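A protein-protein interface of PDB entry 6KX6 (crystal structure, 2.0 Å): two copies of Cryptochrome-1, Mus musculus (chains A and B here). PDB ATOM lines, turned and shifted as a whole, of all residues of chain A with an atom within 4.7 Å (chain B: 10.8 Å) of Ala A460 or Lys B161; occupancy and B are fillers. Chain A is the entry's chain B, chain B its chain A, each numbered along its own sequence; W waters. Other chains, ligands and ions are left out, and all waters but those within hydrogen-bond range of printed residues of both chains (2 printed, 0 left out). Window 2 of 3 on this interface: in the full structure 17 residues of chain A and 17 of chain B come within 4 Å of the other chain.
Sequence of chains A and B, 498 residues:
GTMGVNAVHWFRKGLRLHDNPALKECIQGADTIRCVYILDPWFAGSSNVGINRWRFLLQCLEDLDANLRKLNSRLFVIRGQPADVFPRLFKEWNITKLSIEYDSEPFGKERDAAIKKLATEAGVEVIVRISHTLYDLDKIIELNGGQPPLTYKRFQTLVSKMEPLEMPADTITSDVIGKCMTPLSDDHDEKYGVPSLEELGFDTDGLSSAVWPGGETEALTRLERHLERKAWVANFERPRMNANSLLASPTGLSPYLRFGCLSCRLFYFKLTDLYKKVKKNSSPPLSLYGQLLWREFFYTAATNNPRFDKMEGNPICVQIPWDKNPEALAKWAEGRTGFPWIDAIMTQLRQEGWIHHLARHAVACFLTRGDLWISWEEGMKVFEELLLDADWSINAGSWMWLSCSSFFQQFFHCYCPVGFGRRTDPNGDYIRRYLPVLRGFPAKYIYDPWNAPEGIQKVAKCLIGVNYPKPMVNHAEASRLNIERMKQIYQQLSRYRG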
ATOM      1  N   PRO A 436       0.742  -3.891 -28.152  1.00  0.00           N
ATOM      2  CA  PRO A 436       1.646  -2.826 -28.614  1.00  0.00           C
ATOM      3  C   PRO A 436       2.545  -2.273 -27.527  1.00  0.00           C
ATOM      4  O   PRO A 436       3.611  -1.730 -27.841  1.00  0.00           O
ATOM      5  CB  PRO A 436       0.685  -1.753 -29.150  1.00  0.00           C
ATOM      6  CG  PRO A 436      -0.599  -2.477 -29.423  1.00  0.00           C
ATOM      7  CD  PRO A 436      -0.674  -3.579 -28.413  1.00  0.00           C
ATOM      8  N   VAL A 437       2.162  -2.400 -26.254  1.00  0.00           N
ATOM      9  CA  VAL A 437       3.003  -1.879 -25.184  1.00  0.00           C
ATOM     10  C   VAL A 437       4.333  -2.621 -25.116  1.00  0.00           C
ATOM     11  O   VAL A 437       5.319  -2.082 -24.605  1.00  0.00           O
ATOM     12  CB  VAL A 437       2.248  -1.933 -23.834  1.00  0.00           C
ATOM     13  CG1 VAL A 437       2.216  -3.348 -23.281  1.00  0.00           C
ATOM     14  CG2 VAL A 437       2.865  -0.967 -22.830  1.00  0.00           C
ATOM     15  N   GLY A 440       8.598  -2.522 -28.070  1.00  0.00           N
ATOM     16  CA  GLY A 440      10.005  -2.186 -27.984  1.00  0.00           C
ATOM     17  C   GLY A 440      10.912  -3.319 -27.563  1.00  0.00           C
ATOM     18  O   GLY A 440      12.135  -3.187 -27.677  1.00  0.00           O
ATOM     19  N   PHE A 441      10.346  -4.432 -27.095  1.00  0.00           N
ATOM     20  CA  PHE A 441      11.182  -5.506 -26.578  1.00  0.00           C
ATOM     21  C   PHE A 441      11.808  -6.302 -27.722  1.00  0.00           C
ATOM     22  O   PHE A 441      11.151  -6.563 -28.734  1.00  0.00           O
ATOM     23  CB  PHE A 441      10.371  -6.442 -25.689  1.00  0.00           C
ATOM     24  CG  PHE A 441      10.134  -5.906 -24.308  1.00  0.00           C
ATOM     25  CD1 PHE A 441       9.051  -5.087 -24.045  1.00  0.00           C
ATOM     26  CD2 PHE A 441      10.995  -6.222 -23.273  1.00  0.00           C
ATOM     27  CE1 PHE A 441       8.833  -4.593 -22.775  1.00  0.00           C
ATOM     28  CE2 PHE A 441      10.781  -5.729 -22.001  1.00  0.00           C
ATOM     29  CZ  PHE A 441       9.699  -4.914 -21.752  1.00  0.00           C
ATOM     30  N   ILE A 456      16.777  -2.378 -20.866  1.00  0.00           N
ATOM     31  CA  ILE A 456      15.953  -2.814 -21.987  1.00  0.00           C
ATOM     32  C   ILE A 456      14.523  -2.323 -21.805  1.00  0.00           C
ATOM     33  O   ILE A 456      13.902  -1.796 -22.737  1.00  0.00           O
ATOM     34  CB  ILE A 456      16.012  -4.345 -22.130  1.00  0.00           C
ATOM     35  CG1 ILE A 456      17.458  -4.808 -22.339  1.00  0.00           C
ATOM     36  CG2 ILE A 456      15.120  -4.810 -23.271  1.00  0.00           C
ATOM     37  CD1 ILE A 456      17.974  -4.599 -23.741  1.00  0.00           C
ATOM     38  N   GLN A 457      13.984  -2.478 -20.593  1.00  0.00           N
ATOM     39  CA  GLN A 457      12.616  -2.048 -20.325  1.00  0.00           C
ATOM     40  C   GLN A 457      12.469  -0.539 -20.483  1.00  0.00           C
ATOM     41  O   GLN A 457      11.420  -0.054 -20.926  1.00  0.00           O
ATOM     42  CB  GLN A 457      12.196  -2.486 -18.921  1.00  0.00           C
ATOM     43  CG  GLN A 457      12.168  -3.994 -18.735  1.00  0.00           C
ATOM     44  CD  GLN A 457      11.737  -4.407 -17.340  1.00  0.00           C
ATOM     45  OE1 GLN A 457      10.932  -3.731 -16.699  1.00  0.00           O
ATOM     46  NE2 GLN A 457      12.274  -5.525 -16.864  1.00  0.00           N
ATOM     47  N   LYS A 458      13.514   0.218 -20.136  1.00  0.00           N
ATOM     48  CA  LYS A 458      13.431   1.672 -20.208  1.00  0.00           C
ATOM     49  C   LYS A 458      13.421   2.153 -21.653  1.00  0.00           C
ATOM     50  O   LYS A 458      12.620   3.019 -22.025  1.00  0.00           O
ATOM     51  CB  LYS A 458      14.588   2.307 -19.435  1.00  0.00           C
ATOM     52  CG  LYS A 458      14.341   2.407 -17.935  1.00  0.00           C
ATOM     53  CD  LYS A 458      15.551   2.956 -17.183  1.00  0.00           C
ATOM     54  CE  LYS A 458      16.274   4.037 -17.976  1.00  0.00           C
ATOM     55  NZ  LYS A 458      16.804   5.122 -17.102  1.00  0.00           N
ATOM     56  N   VAL A 459      14.311   1.609 -22.488  1.00  0.00           N
ATOM     57  CA  VAL A 459      14.310   1.976 -23.900  1.00  0.00           C
ATOM     58  C   VAL A 459      13.010   1.534 -24.562  1.00  0.00           C
ATOM     59  O   VAL A 459      12.486   2.224 -25.446  1.00  0.00           O
ATOM     60  CB  VAL A 459      15.551   1.386 -24.599  1.00  0.00           C
ATOM     61  CG1 VAL A 459      15.313   1.218 -26.093  1.00  0.00           C
ATOM     62  CG2 VAL A 459      16.762   2.271 -24.347  1.00  0.00           C
ATOM     63  N   ALA A 460      12.457   0.399 -24.135  1.00  0.00           N
ATOM     64  CA  ALA A 460      11.167  -0.044 -24.649  1.00  0.00           C
ATOM     65  C   ALA A 460      10.003   0.744 -24.068  1.00  0.00           C
ATOM     66  O   ALA A 460       8.869   0.569 -24.528  1.00  0.00           O
ATOM     67  CB  ALA A 460      10.975  -1.535 -24.366  1.00  0.00           C
ATOM     68  N   LYS A 461      10.257   1.599 -23.073  1.00  0.00           N
ATOM     69  CA  LYS A 461       9.220   2.410 -22.433  1.00  0.00           C
ATOM     70  C   LYS A 461       8.112   1.539 -21.846  1.00  0.00           C
ATOM     71  O   LYS A 461       6.930   1.885 -21.902  1.00  0.00           O
ATOM     72  CB  LYS A 461       8.639   3.440 -23.408  1.00  0.00           C
ATOM     73  CG  LYS A 461       9.625   4.504 -23.850  1.00  0.00           C
ATOM     74  CD  LYS A 461       8.933   5.841 -24.050  1.00  0.00           C
ATOM     75  CE  LYS A 461       9.873   6.994 -23.740  1.00  0.00           C
ATOM     76  NZ  LYS A 461      11.089   6.962 -24.600  1.00  0.00           N
ATOM     77  N   CYS A 462       8.493   0.396 -21.274  1.00  0.00           N
ATOM     78  CA  CYS A 462       7.511  -0.504 -20.671  1.00  0.00           C
ATOM     79  C   CYS A 462       8.162  -1.163 -19.458  1.00  0.00           C
ATOM     80  O   CYS A 462       8.932  -2.117 -19.604  1.00  0.00           O
ATOM     81  CB  CYS A 462       7.032  -1.541 -21.677  1.00  0.00           C
ATOM     82  SG  CYS A 462       5.863  -2.741 -21.000  1.00  0.00           S
ATOM     83  N   ASN A 467       3.727  -0.812 -16.588  1.00  0.00           N
ATOM     84  CA  ASN A 467       3.040  -0.627 -17.860  1.00  0.00           C
ATOM     85  C   ASN A 467       2.489  -1.923 -18.434  1.00  0.00           C
ATOM     86  O   ASN A 467       1.666  -1.877 -19.358  1.00  0.00           O
ATOM     87  CB  ASN A 467       3.983   0.013 -18.878  1.00  0.00           C
ATOM     88  CG  ASN A 467       4.687   1.232 -18.326  1.00  0.00           C
ATOM     89  OD1 ASN A 467       5.803   1.136 -17.817  1.00  0.00           O
ATOM     90  ND2 ASN A 467       4.037   2.387 -18.423  1.00  0.00           N
ATOM     91  N   TYR B 135      -2.854  14.121 -18.606  1.00  0.00           N
ATOM     92  CA  TYR B 135      -1.481  14.110 -19.079  1.00  0.00           C
ATOM     93  C   TYR B 135      -1.101  15.461 -19.663  1.00  0.00           C
ATOM     94  O   TYR B 135      -1.952  16.301 -19.972  1.00  0.00           O
ATOM     95  CB  TYR B 135      -1.267  13.027 -20.143  1.00  0.00           C
ATOM     96  CG  TYR B 135      -1.476  11.622 -19.638  1.00  0.00           C
ATOM     97  CD1 TYR B 135      -0.501  10.986 -18.879  1.00  0.00           C
ATOM     98  CD2 TYR B 135      -2.644  10.929 -19.919  1.00  0.00           C
ATOM     99  CE1 TYR B 135      -0.684   9.700 -18.413  1.00  0.00           C
ATOM    100  CE2 TYR B 135      -2.839   9.641 -19.458  1.00  0.00           C
ATOM    101  CZ  TYR B 135      -1.855   9.032 -18.706  1.00  0.00           C
ATOM    102  OH  TYR B 135      -2.045   7.750 -18.243  1.00  0.00           O
ATOM    103  N   LYS B 139       3.556  16.390 -24.314  1.00  0.00           N
ATOM    104  CA  LYS B 139       4.403  15.213 -24.155  1.00  0.00           C
ATOM    105  C   LYS B 139       3.832  14.012 -24.899  1.00  0.00           C
ATOM    106  O   LYS B 139       4.591  13.172 -25.397  1.00  0.00           O
ATOM    107  CB  LYS B 139       4.579  14.890 -22.671  1.00  0.00           C
ATOM    108  CG  LYS B 139       6.028  14.755 -22.230  1.00  0.00           C
ATOM    109  CD  LYS B 139       6.139  14.583 -20.721  1.00  0.00           C
ATOM    110  CE  LYS B 139       6.413  15.909 -20.024  1.00  0.00           C
ATOM    111  NZ  LYS B 139       7.031  15.717 -18.681  1.00  0.00           N
ATOM    112  N   ILE B 140       2.503  13.916 -24.982  1.00  0.00           N
ATOM    113  CA  ILE B 140       1.879  12.874 -25.792  1.00  0.00           C
ATOM    114  C   ILE B 140       2.237  13.066 -27.256  1.00  0.00           C
ATOM    115  O   ILE B 140       2.647  12.127 -27.947  1.00  0.00           O
ATOM    116  CB  ILE B 140       0.354  12.873 -25.595  1.00  0.00           C
ATOM    117  CG1 ILE B 140      -0.004  12.701 -24.119  1.00  0.00           C
ATOM    118  CG2 ILE B 140      -0.289  11.779 -26.444  1.00  0.00           C
ATOM    119  CD1 ILE B 140      -1.454  12.312 -23.892  1.00  0.00           C
ATOM    120  N   GLU B 142       4.685  14.785 -28.552  1.00  0.00           N
ATOM    121  CA  GLU B 142       6.114  14.561 -28.754  1.00  0.00           C
ATOM    122  C   GLU B 142       6.430  13.073 -28.857  1.00  0.00           C
ATOM    123  O   GLU B 142       7.204  12.657 -29.727  1.00  0.00           O
ATOM    124  CB  GLU B 142       6.914  15.205 -27.621  1.00  0.00           C
ATOM    125  N   LEU B 143       5.832  12.257 -27.985  1.00  0.00           N
ATOM    126  CA  LEU B 143       6.045  10.813 -28.051  1.00  0.00           C
ATOM    127  C   LEU B 143       5.563  10.232 -29.375  1.00  0.00           C
ATOM    128  O   LEU B 143       6.161   9.280 -29.887  1.00  0.00           O
ATOM    129  CB  LEU B 143       5.340  10.123 -26.885  1.00  0.00           C
ATOM    130  N   ASN B 144       4.493  10.790 -29.945  1.00  0.00           N
ATOM    131  CA  ASN B 144       3.963  10.317 -31.217  1.00  0.00           C
ATOM    132  C   ASN B 144       4.733  10.850 -32.418  1.00  0.00           C
ATOM    133  O   ASN B 144       4.398  10.494 -33.552  1.00  0.00           O
ATOM    134  CB  ASN B 144       2.484  10.699 -31.346  1.00  0.00           C
ATOM    135  CG  ASN B 144       1.731   9.802 -32.312  1.00  0.00           C
ATOM    136  OD1 ASN B 144       1.837   8.578 -32.253  1.00  0.00           O
ATOM    137  ND2 ASN B 144       0.966  10.412 -33.211  1.00  0.00           N
ATOM    138  N   LYS B 153      -6.822   3.734 -30.751  1.00  0.00           N
ATOM    139  CA  LYS B 153      -5.973   2.601 -30.401  1.00  0.00           C
ATOM    140  C   LYS B 153      -4.525   3.035 -30.222  1.00  0.00           C
ATOM    141  O   LYS B 153      -3.853   2.602 -29.278  1.00  0.00           O
ATOM    142  CB  LYS B 153      -6.081   1.513 -31.470  1.00  0.00           C
ATOM    143  N   ARG B 154      -4.027   3.891 -31.118  1.00  0.00           N
ATOM    144  CA  ARG B 154      -2.676   4.415 -30.963  1.00  0.00           C
ATOM    145  C   ARG B 154      -2.568   5.287 -29.718  1.00  0.00           C
ATOM    146  O   ARG B 154      -1.539   5.276 -29.032  1.00  0.00           O
ATOM    147  CB  ARG B 154      -2.271   5.202 -32.211  1.00  0.00           C
ATOM    148  N   PHE B 155      -3.623   6.044 -29.408  1.00  0.00           N
ATOM    149  CA  PHE B 155      -3.616   6.865 -28.201  1.00  0.00           C
ATOM    150  C   PHE B 155      -3.506   6.000 -26.951  1.00  0.00           C
ATOM    151  O   PHE B 155      -2.773   6.339 -26.016  1.00  0.00           O
ATOM    152  CB  PHE B 155      -4.875   7.730 -28.155  1.00  0.00           C
ATOM    153  CG  PHE B 155      -4.949   8.634 -26.957  1.00  0.00           C
ATOM    154  CD1 PHE B 155      -4.288   9.851 -26.952  1.00  0.00           C
ATOM    155  CD2 PHE B 155      -5.689   8.274 -25.843  1.00  0.00           C
ATOM    156  CE1 PHE B 155      -4.355  10.686 -25.856  1.00  0.00           C
ATOM    157  CE2 PHE B 155      -5.762   9.107 -24.745  1.00  0.00           C
ATOM    158  CZ  PHE B 155      -5.091  10.312 -24.751  1.00  0.00           C
ATOM    159  N   GLN B 156      -4.231   4.878 -26.917  1.00  0.00           N
ATOM    160  CA  GLN B 156      -4.105   3.945 -25.802  1.00  0.00           C
ATOM    161  C   GLN B 156      -2.689   3.402 -25.697  1.00  0.00           C
ATOM    162  O   GLN B 156      -2.153   3.251 -24.593  1.00  0.00           O
ATOM    163  CB  GLN B 156      -5.097   2.793 -25.962  1.00  0.00           C
ATOM    164  CG  GLN B 156      -6.508   3.111 -25.519  1.00  0.00           C
ATOM    165  CD  GLN B 156      -7.389   1.879 -25.485  1.00  0.00           C
ATOM    166  OE1 GLN B 156      -8.040   1.593 -24.480  1.00  0.00           O
ATOM    167  NE2 GLN B 156      -7.409   1.139 -26.585  1.00  0.00           N
ATOM    168  N   THR B 157      -2.073   3.088 -26.839  1.00  0.00           N
ATOM    169  CA  THR B 157      -0.699   2.600 -26.835  1.00  0.00           C
ATOM    170  C   THR B 157       0.251   3.645 -26.263  1.00  0.00           C
ATOM    171  O   THR B 157       1.145   3.319 -25.473  1.00  0.00           O
ATOM    172  CB  THR B 157      -0.286   2.209 -28.256  1.00  0.00           C
ATOM    173  OG1 THR B 157      -1.101   1.121 -28.703  1.00  0.00           O
ATOM    174  CG2 THR B 157       1.180   1.794 -28.301  1.00  0.00           C
ATOM    175  N   LEU B 158       0.061   4.910 -26.639  1.00  0.00           N
ATOM    176  CA  LEU B 158       0.890   5.977 -26.090  1.00  0.00           C
ATOM    177  C   LEU B 158       0.666   6.132 -24.591  1.00  0.00           C
ATOM    178  O   LEU B 158       1.622   6.306 -23.825  1.00  0.00           O
ATOM    179  CB  LEU B 158       0.592   7.290 -26.810  1.00  0.00           C
ATOM    180  CG  LEU B 158       1.222   7.492 -28.187  1.00  0.00           C
ATOM    181  CD1 LEU B 158       0.499   8.601 -28.935  1.00  0.00           C
ATOM    182  CD2 LEU B 158       2.702   7.811 -28.056  1.00  0.00           C
ATOM    183  N   VAL B 159      -0.593   6.056 -24.152  1.00  0.00           N
ATOM    184  CA  VAL B 159      -0.912   6.299 -22.749  1.00  0.00           C
ATOM    185  C   VAL B 159      -0.343   5.194 -21.867  1.00  0.00           C
ATOM    186  O   VAL B 159       0.137   5.452 -20.756  1.00  0.00           O
ATOM    187  CB  VAL B 159      -2.437   6.439 -22.579  1.00  0.00           C
ATOM    188  CG1 VAL B 159      -2.835   6.339 -21.111  1.00  0.00           C
ATOM    189  CG2 VAL B 159      -2.896   7.762 -23.170  1.00  0.00           C
ATOM    190  N   SER B 160      -0.370   3.952 -22.350  1.00  0.00           N
ATOM    191  CA  SER B 160       0.142   2.836 -21.567  1.00  0.00           C
ATOM    192  C   SER B 160       1.657   2.863 -21.422  1.00  0.00           C
ATOM    193  O   SER B 160       2.193   2.122 -20.591  1.00  0.00           O
ATOM    194  CB  SER B 160      -0.290   1.519 -22.206  1.00  0.00           C
ATOM    195  OG  SER B 160       0.360   1.338 -23.451  1.00  0.00           O
ATOM    196  N   LYS B 161       2.355   3.689 -22.202  1.00  0.00           N
ATOM    197  CA  LYS B 161       3.801   3.822 -22.110  1.00  0.00           C
ATOM    198  C   LYS B 161       4.241   5.001 -21.253  1.00  0.00           C
ATOM    199  O   LYS B 161       5.443   5.156 -21.015  1.00  0.00           O
ATOM    200  CB  LYS B 161       4.417   3.968 -23.507  1.00  0.00           C
ATOM    201  CG  LYS B 161       4.385   2.704 -24.345  1.00  0.00           C
ATOM    202  CD  LYS B 161       5.568   2.675 -25.297  1.00  0.00           C
ATOM    203  CE  LYS B 161       5.134   2.358 -26.715  1.00  0.00           C
ATOM    204  NZ  LYS B 161       6.123   1.491 -27.416  1.00  0.00           N
ATOM    205  N   MET B 162       3.310   5.831 -20.790  1.00  0.00           N
ATOM    206  CA  MET B 162       3.669   6.999 -20.006  1.00  0.00           C
ATOM    207  C   MET B 162       3.981   6.606 -18.566  1.00  0.00           C
ATOM    208  O   MET B 162       3.631   5.519 -18.097  1.00  0.00           O
ATOM    209  CB  MET B 162       2.546   8.038 -20.033  1.00  0.00           C
ATOM    210  CG  MET B 162       2.231   8.531 -21.431  1.00  0.00           C
ATOM    211  SD  MET B 162       3.236   9.966 -21.839  1.00  0.00           S
ATOM    212  CE  MET B 162       2.519  10.473 -23.393  1.00  0.00           C
ATOM    213  N   GLU B 163       4.657   7.514 -17.871  1.00  0.00           N
ATOM    214  CA  GLU B 163       4.955   7.306 -16.467  1.00  0.00           C
ATOM    215  C   GLU B 163       3.659   7.283 -15.658  1.00  0.00           C
ATOM    216  O   GLU B 163       2.653   7.868 -16.068  1.00  0.00           O
ATOM    217  CB  GLU B 163       5.878   8.410 -15.951  1.00  0.00           C
ATOM    218  N   PRO B 164       3.649   6.593 -14.516  1.00  0.00           N
ATOM    219  CA  PRO B 164       2.452   6.597 -13.669  1.00  0.00           C
ATOM    220  C   PRO B 164       2.102   8.006 -13.215  1.00  0.00           C
ATOM    221  O   PRO B 164       2.975   8.854 -13.008  1.00  0.00           O
ATOM    222  CB  PRO B 164       2.848   5.710 -12.483  1.00  0.00           C
ATOM    223  CG  PRO B 164       3.953   4.864 -12.997  1.00  0.00           C
ATOM    224  CD  PRO B 164       4.700   5.712 -13.980  1.00  0.00           C
ATOM    225  N   LEU B 165       0.804   8.250 -13.071  1.00  0.00           N
ATOM    226  CA  LEU B 165       0.331   9.565 -12.666  1.00  0.00           C
ATOM    227  C   LEU B 165       0.765   9.879 -11.241  1.00  0.00           C
ATOM    228  O   LEU B 165       0.565   9.076 -10.325  1.00  0.00           O
ATOM    229  CB  LEU B 165      -1.191   9.632 -12.775  1.00  0.00           C
ATOM    230  CG  LEU B 165      -1.767   9.699 -14.188  1.00  0.00           C
ATOM    231  CD1 LEU B 165      -3.197   9.199 -14.206  1.00  0.00           C
ATOM    232  CD2 LEU B 165      -1.695  11.118 -14.705  1.00  0.00           C
ATOM    233  N   TYR B 268      -9.580   9.683 -11.412  1.00  0.00           N
ATOM    234  CA  TYR B 268      -8.696   8.587 -11.795  1.00  0.00           C
ATOM    235  C   TYR B 268      -8.246   7.793 -10.577  1.00  0.00           C
ATOM    236  O   TYR B 268      -8.288   6.557 -10.574  1.00  0.00           O
ATOM    237  CB  TYR B 268      -7.486   9.145 -12.555  1.00  0.00           C
ATOM    238  CG  TYR B 268      -6.595   8.099 -13.196  1.00  0.00           C
ATOM    239  CD1 TYR B 268      -5.703   7.350 -12.434  1.00  0.00           C
ATOM    240  CD2 TYR B 268      -6.635   7.872 -14.565  1.00  0.00           C
ATOM    241  CE1 TYR B 268      -4.889   6.397 -13.016  1.00  0.00           C
ATOM    242  CE2 TYR B 268      -5.820   6.921 -15.157  1.00  0.00           C
ATOM    243  CZ  TYR B 268      -4.949   6.188 -14.376  1.00  0.00           C
ATOM    244  OH  TYR B 268      -4.135   5.243 -14.955  1.00  0.00           O
ATOM    245  N   LEU B 286      -7.336  -0.346 -19.259  1.00  0.00           N
ATOM    246  CA  LEU B 286      -7.611   1.061 -19.529  1.00  0.00           C
ATOM    247  C   LEU B 286      -9.106   1.316 -19.633  1.00  0.00           C
ATOM    248  O   LEU B 286      -9.565   2.433 -19.366  1.00  0.00           O
ATOM    249  CB  LEU B 286      -6.900   1.512 -20.807  1.00  0.00           C
ATOM    250  CG  LEU B 286      -5.378   1.668 -20.728  1.00  0.00           C
ATOM    251  CD1 LEU B 286      -4.868   2.612 -21.809  1.00  0.00           C
ATOM    252  CD2 LEU B 286      -4.941   2.147 -19.347  1.00  0.00           C
ATOM    253  N   LEU B 293     -10.097   8.768 -20.783  1.00  0.00           N
ATOM    254  CA  LEU B 293      -9.171   8.739 -21.914  1.00  0.00           C
ATOM    255  C   LEU B 293      -9.797   9.253 -23.202  1.00  0.00           C
ATOM    256  O   LEU B 293      -9.077   9.785 -24.057  1.00  0.00           O
ATOM    257  CB  LEU B 293      -8.618   7.330 -22.156  1.00  0.00           C
ATOM    258  CG  LEU B 293      -7.600   6.749 -21.164  1.00  0.00           C
ATOM    259  CD1 LEU B 293      -6.369   7.644 -21.023  1.00  0.00           C
ATOM    260  CD2 LEU B 293      -8.212   6.480 -19.810  1.00  0.00           C
HETATM  261  O   HOH W   1       7.432  -1.164 -26.068  1.00  0.00           O
HETATM  262  O   HOH W   2       4.061   0.598 -29.673  1.00  0.00           O
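Among the printed residues, pairs that only touch across the chains: Pro A436 with Thr B157 (3.4 Å), Val A437 with Ser B160 (3.5 Å), Lys A461 with Lys B161 (3.6 Å), Asn A467 with Lys B161 (3.9 Å) and Ala A460 with Lys B161 (3.99 Å).
No position is printed for both chains.
Among the printed residues, 7 pairs touch across the chains.
O of Ser B160 sits at hydrogen-bond distance from ND2 of Asn A467, at 2.9 Å.
O of Met B162 lies within hydrogen-bond range of ND2 of Asn A467, 3.2 Å away.
Water W1 lies within hydrogen-bond range of the backbone NH of Gly A440, the backbone carbonyl oxygen of Ala A460, the backbone carbonyl oxygen of Val A437 and the side-chain amino group of Lys B161.
Water W2 bridges O of Pro A436 (3.0 Å) and NZ of Lys B161 (3.2 Å).
O of Lys B153 is in hydrogen-bond range of OG1 of Thr B157, at 3.2 Å.
O of Gln B156 sits at hydrogen-bond distance from OG of Ser B160.
The backbone carbonyl oxygen of Thr B157 is in hydrogen-bond range of the side-chain hydroxyl of Ser B160 (2.9 Å).
The side-chain sulfur (SG) of Cys A462 lies close to the backbone carbonyl oxygen (O) of Val A437 (3.7 Å).
Printed residues of chain B within 4 Å of Ala A460: Lys B161 (3.99 Å).
Of the printed residues of chain A, Lys B161 touches Ala A460, Lys A461 and Asn A467.
Val A437 touches one residue of chain B.
No residue of chain B comes within 4 Å of Phe A441.
No residue of chain B comes within 4 Å of Val A459.
No residue of chain B comes within 4 Å of Cys A462.
Printed residues of chain B within 4 Å of Asn A467: Ser B160, Lys B161 and Met B162.
Printed residues of chain B within 4 Å of Pro A436: Thr B157.
Of the printed residues of chain A, Met B162 touches Asn A467 (3.2 Å).
Tyr B268 touches none of the printed residues of chain A.
Leu B165 touches none of the printed residues of chain A.
The nearest printed residue of chain B that does not touch Ala A460 is Ser B160 (7.9 Å).
The nearest printed residue of chain B that does not touch Asn A467 is Glu B163 (5.2 Å).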
